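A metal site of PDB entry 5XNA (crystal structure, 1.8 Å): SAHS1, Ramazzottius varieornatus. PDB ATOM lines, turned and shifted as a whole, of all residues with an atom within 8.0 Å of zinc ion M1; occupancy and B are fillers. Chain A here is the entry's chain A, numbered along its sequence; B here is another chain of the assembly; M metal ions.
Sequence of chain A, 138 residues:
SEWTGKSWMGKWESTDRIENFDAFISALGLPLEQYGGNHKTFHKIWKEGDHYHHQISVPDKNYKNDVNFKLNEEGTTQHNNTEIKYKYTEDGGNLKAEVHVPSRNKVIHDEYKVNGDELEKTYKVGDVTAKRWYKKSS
Zinc ion M1 is bound by a ring nitrogen (NE2) of His 109 of chain A, at 1.9 Å.
OE2 of Glu 98 of chain B is bound to zinc ion M1, at 2.0 Å.
NE2 of His 109 of chain B binds zinc ion M1 (2.0 Å).
OE2 of Glu 98 of chain A is bound to zinc ion M1.
Slightly farther from zinc ion M1 lies OE1 of Glu 98 of chain A (2.7 Å).
A ring nitrogen (NE2) of His 100 of chain B lies close to the side-chain carboxylate of Glu 98 of chain B.
N of His 109 of chain A lies within hydrogen-bond range of O of Lys 124.
Val 107 of chain B touches zinc ion M1 (CG1 to ZN, 3.8 Å).
Within 4 Å of zinc ion M1: Glu 98 of chain A, His 109 of chain A, Glu 98 of chain B, Val 107 of chain B and His 109 of chain B.
The nearest printed residue that does not touch zinc ion M1 is His 100 of chain B (4.1 Å).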
ATOM      1  N   ALA A  97      -7.187  20.304  11.464  1.00  0.00           N
ATOM      2  CA  ALA A  97      -5.999  21.015  11.028  1.00  0.00           C
ATOM      3  C   ALA A  97      -4.795  20.499  11.808  1.00  0.00           C
ATOM      4  O   ALA A  97      -4.858  20.386  13.045  1.00  0.00           O
ATOM      5  CB  ALA A  97      -6.143  22.526  11.217  1.00  0.00           C
ATOM      6  N   GLU A  98      -3.726  20.191  11.089  1.00  0.00           N
ATOM      7  CA  GLU A  98      -2.427  19.815  11.649  1.00  0.00           C
ATOM      8  C   GLU A  98      -1.510  21.030  11.568  1.00  0.00           C
ATOM      9  O   GLU A  98      -1.252  21.513  10.465  1.00  0.00           O
ATOM     10  CB  GLU A  98      -1.828  18.640  10.880  1.00  0.00           C
ATOM     11  CG  GLU A  98      -0.561  18.093  11.510  1.00  0.00           C
ATOM     12  CD  GLU A  98      -0.862  17.057  12.590  1.00  0.00           C
ATOM     13  OE1 GLU A  98      -2.039  16.652  12.716  1.00  0.00           O
ATOM     14  OE2 GLU A  98       0.081  16.674  13.292  1.00  0.00           O
ATOM     15  N   VAL A  99      -1.051  21.537  12.709  1.00  0.00           N
ATOM     16  CA  VAL A  99      -0.328  22.810  12.738  1.00  0.00           C
ATOM     17  C   VAL A  99       1.068  22.590  13.313  1.00  0.00           C
ATOM     18  O   VAL A  99       1.212  22.054  14.413  1.00  0.00           O
ATOM     19  CB  VAL A  99      -1.092  23.862  13.557  1.00  0.00           C
ATOM     20  CG1 VAL A  99      -0.312  25.178  13.591  1.00  0.00           C
ATOM     21  CG2 VAL A  99      -2.487  24.064  12.984  1.00  0.00           C
ATOM     22  N   HIS A 100       2.090  23.002  12.564  1.00  0.00           N
ATOM     23  CA  HIS A 100       3.469  23.016  13.065  1.00  0.00           C
ATOM     24  C   HIS A 100       3.850  24.430  13.464  1.00  0.00           C
ATOM     25  O   HIS A 100       3.620  25.382  12.712  1.00  0.00           O
ATOM     26  CB  HIS A 100       4.465  22.527  12.007  1.00  0.00           C
ATOM     27  CG  HIS A 100       4.483  21.037  11.771  1.00  0.00           C
ATOM     28  ND1 HIS A 100       3.524  20.387  11.022  1.00  0.00           N
ATOM     29  CD2 HIS A 100       5.391  20.099  12.127  1.00  0.00           C
ATOM     30  CE1 HIS A 100       3.830  19.103  10.942  1.00  0.00           C
ATOM     31  NE2 HIS A 100       4.958  18.903  11.610  1.00  0.00           N
ATOM     32  N   VAL A 107       3.532  20.944  17.948  1.00  0.00           N
ATOM     33  CA  VAL A 107       2.538  20.440  16.996  1.00  0.00           C
ATOM     34  C   VAL A 107       1.161  20.584  17.638  1.00  0.00           C
ATOM     35  O   VAL A 107       0.928  20.068  18.739  1.00  0.00           O
ATOM     36  CB  VAL A 107       2.808  18.985  16.601  1.00  0.00           C
ATOM     37  CG1 VAL A 107       1.684  18.476  15.689  1.00  0.00           C
ATOM     38  CG2 VAL A 107       4.173  18.834  15.933  1.00  0.00           C
ATOM     39  N   ILE A 108       0.255  21.282  16.957  1.00  0.00           N
ATOM     40  CA  ILE A 108      -1.084  21.562  17.480  1.00  0.00           C
ATOM     41  C   ILE A 108      -2.102  20.846  16.606  1.00  0.00           C
ATOM     42  O   ILE A 108      -1.989  20.881  15.373  1.00  0.00           O
ATOM     43  CB  ILE A 108      -1.389  23.074  17.497  1.00  0.00           C
ATOM     44  CG1 ILE A 108      -0.405  23.835  18.373  1.00  0.00           C
ATOM     45  CG2 ILE A 108      -2.836  23.321  17.915  1.00  0.00           C
ATOM     46  CD1 ILE A 108      -0.463  25.328  18.179  1.00  0.00           C
ATOM     47  N   HIS A 109      -3.041  20.156  17.235  1.00  0.00           N
ATOM     48  CA  HIS A 109      -4.206  19.619  16.545  1.00  0.00           C
ATOM     49  C   HIS A 109      -5.402  20.531  16.773  1.00  0.00           C
ATOM     50  O   HIS A 109      -5.699  20.887  17.919  1.00  0.00           O
ATOM     51  CB  HIS A 109      -4.556  18.203  17.035  1.00  0.00           C
ATOM     52  CG  HIS A 109      -3.584  17.155  16.609  1.00  0.00           C
ATOM     53  ND1 HIS A 109      -3.637  15.864  17.080  1.00  0.00           N
ATOM     54  CD2 HIS A 109      -2.549  17.197  15.741  1.00  0.00           C
ATOM     55  CE1 HIS A 109      -2.657  15.153  16.536  1.00  0.00           C
ATOM     56  NE2 HIS A 109      -1.972  15.943  15.723  1.00  0.00           N
ATOM     57  N   ASP A 110      -6.085  20.906  15.692  1.00  0.00           N
ATOM     58  CA  ASP A 110      -7.391  21.544  15.749  1.00  0.00           C
ATOM     59  C   ASP A 110      -8.421  20.585  15.175  1.00  0.00           C
ATOM     60  O   ASP A 110      -8.135  19.887  14.190  1.00  0.00           O
ATOM     61  CB  ASP A 110      -7.436  22.832  14.934  1.00  0.00           C
ATOM     62  CG  ASP A 110      -6.518  23.887  15.447  1.00  0.00           C
ATOM     63  OD1 ASP A 110      -6.305  23.927  16.673  1.00  0.00           O
ATOM     64  OD2 ASP A 110      -6.012  24.672  14.623  1.00  0.00           O
ATOM     65  N   LYS A 124      -5.518  20.607  20.795  1.00  0.00           N
ATOM     66  CA  LYS A 124      -4.709  19.608  21.483  1.00  0.00           C
ATOM     67  C   LYS A 124      -3.240  19.795  21.162  1.00  0.00           C
ATOM     68  O   LYS A 124      -2.850  19.854  19.997  1.00  0.00           O
ATOM     69  CB  LYS A 124      -5.149  18.191  21.100  1.00  0.00           C
ATOM     70  CG  LYS A 124      -4.558  17.102  21.965  1.00  0.00           C
ATOM     71  CD  LYS A 124      -5.111  15.742  21.566  1.00  0.00           C
ATOM     72  CE  LYS A 124      -6.629  15.777  21.439  1.00  0.00           C
ATOM     73  NZ  LYS A 124      -7.198  14.460  20.997  1.00  0.00           N
ATOM     74  N   ALA B  97       0.178   7.279  19.148  1.00  0.00           N
ATOM     75  CA  ALA B  97       1.532   7.684  18.789  1.00  0.00           C
ATOM     76  C   ALA B  97       1.457   8.775  17.724  1.00  0.00           C
ATOM     77  O   ALA B  97       0.740   8.625  16.723  1.00  0.00           O
ATOM     78  CB  ALA B  97       2.353   6.497  18.269  1.00  0.00           C
ATOM     79  N   GLU B  98       2.133   9.881  17.975  1.00  0.00           N
ATOM     80  CA  GLU B  98       2.270  10.995  17.043  1.00  0.00           C
ATOM     81  C   GLU B  98       3.625  10.826  16.384  1.00  0.00           C
ATOM     82  O   GLU B  98       4.647  10.892  17.061  1.00  0.00           O
ATOM     83  CB  GLU B  98       2.199  12.314  17.803  1.00  0.00           C
ATOM     84  CG  GLU B  98       2.335  13.558  16.943  1.00  0.00           C
ATOM     85  CD  GLU B  98       1.045  13.911  16.254  1.00  0.00           C
ATOM     86  OE1 GLU B  98      -0.026  13.384  16.651  1.00  0.00           O
ATOM     87  OE2 GLU B  98       1.103  14.713  15.306  1.00  0.00           O
ATOM     88  N   VAL B  99       3.644  10.541  15.081  1.00  0.00           N
ATOM     89  CA  VAL B  99       4.891  10.106  14.436  1.00  0.00           C
ATOM     90  C   VAL B  99       5.165  11.062  13.285  1.00  0.00           C
ATOM     91  O   VAL B  99       4.360  11.153  12.349  1.00  0.00           O
ATOM     92  CB  VAL B  99       4.787   8.662  13.943  1.00  0.00           C
ATOM     93  CG1 VAL B  99       6.062   8.244  13.243  1.00  0.00           C
ATOM     94  CG2 VAL B  99       4.456   7.722  15.136  1.00  0.00           C
ATOM     95  N   HIS B 100       6.280  11.767  13.352  1.00  0.00           N
ATOM     96  CA  HIS B 100       6.634  12.732  12.326  1.00  0.00           C
ATOM     97  C   HIS B 100       7.919  12.304  11.640  1.00  0.00           C
ATOM     98  O   HIS B 100       8.886  11.880  12.291  1.00  0.00           O
ATOM     99  CB  HIS B 100       6.760  14.135  12.904  1.00  0.00           C
ATOM    100  CG  HIS B 100       5.453  14.742  13.327  1.00  0.00           C
ATOM    101  ND1 HIS B 100       5.045  15.983  12.929  1.00  0.00           N
ATOM    102  CD2 HIS B 100       4.456  14.241  14.105  1.00  0.00           C
ATOM    103  CE1 HIS B 100       3.854  16.253  13.446  1.00  0.00           C
ATOM    104  NE2 HIS B 100       3.482  15.210  14.171  1.00  0.00           N
ATOM    105  N   VAL B 107       3.274  13.000   8.392  1.00  0.00           N
ATOM    106  CA  VAL B 107       2.765  12.891   9.747  1.00  0.00           C
ATOM    107  C   VAL B 107       1.879  11.665   9.810  1.00  0.00           C
ATOM    108  O   VAL B 107       0.916  11.552   9.034  1.00  0.00           O
ATOM    109  CB  VAL B 107       1.969  14.139  10.175  1.00  0.00           C
ATOM    110  CG1 VAL B 107       1.387  13.906  11.582  1.00  0.00           C
ATOM    111  CG2 VAL B 107       2.840  15.377  10.150  1.00  0.00           C
ATOM    112  N   ILE B 108       2.161  10.771  10.744  1.00  0.00           N
ATOM    113  CA  ILE B 108       1.379   9.556  10.927  1.00  0.00           C
ATOM    114  C   ILE B 108       0.732   9.643  12.307  1.00  0.00           C
ATOM    115  O   ILE B 108       1.415   9.975  13.281  1.00  0.00           O
ATOM    116  CB  ILE B 108       2.266   8.297  10.823  1.00  0.00           C
ATOM    117  CG1 ILE B 108       2.951   8.247   9.458  1.00  0.00           C
ATOM    118  CG2 ILE B 108       1.441   7.040  11.157  1.00  0.00           C
ATOM    119  CD1 ILE B 108       4.209   7.417   9.439  1.00  0.00           C
ATOM    120  N   HIS B 109      -0.559   9.368  12.371  1.00  0.00           N
ATOM    121  CA  HIS B 109      -1.290   9.243  13.637  1.00  0.00           C
ATOM    122  C   HIS B 109      -1.648   7.774  13.852  1.00  0.00           C
ATOM    123  O   HIS B 109      -2.454   7.225  13.105  1.00  0.00           O
ATOM    124  CB  HIS B 109      -2.573  10.082  13.638  1.00  0.00           C
ATOM    125  CG  HIS B 109      -2.329  11.558  13.609  1.00  0.00           C
ATOM    126  ND1 HIS B 109      -3.292  12.456  13.206  1.00  0.00           N
ATOM    127  CD2 HIS B 109      -1.256  12.303  13.981  1.00  0.00           C
ATOM    128  CE1 HIS B 109      -2.807  13.683  13.285  1.00  0.00           C
ATOM    129  NE2 HIS B 109      -1.578  13.619  13.753  1.00  0.00           N
HETATM  130 ZN    ZN M   1      -0.646  15.217  14.517  1.00  0.00          ZN
HETATM  131 ZN    ZN M   2       6.122  17.284  11.679  1.00  0.00          ZN
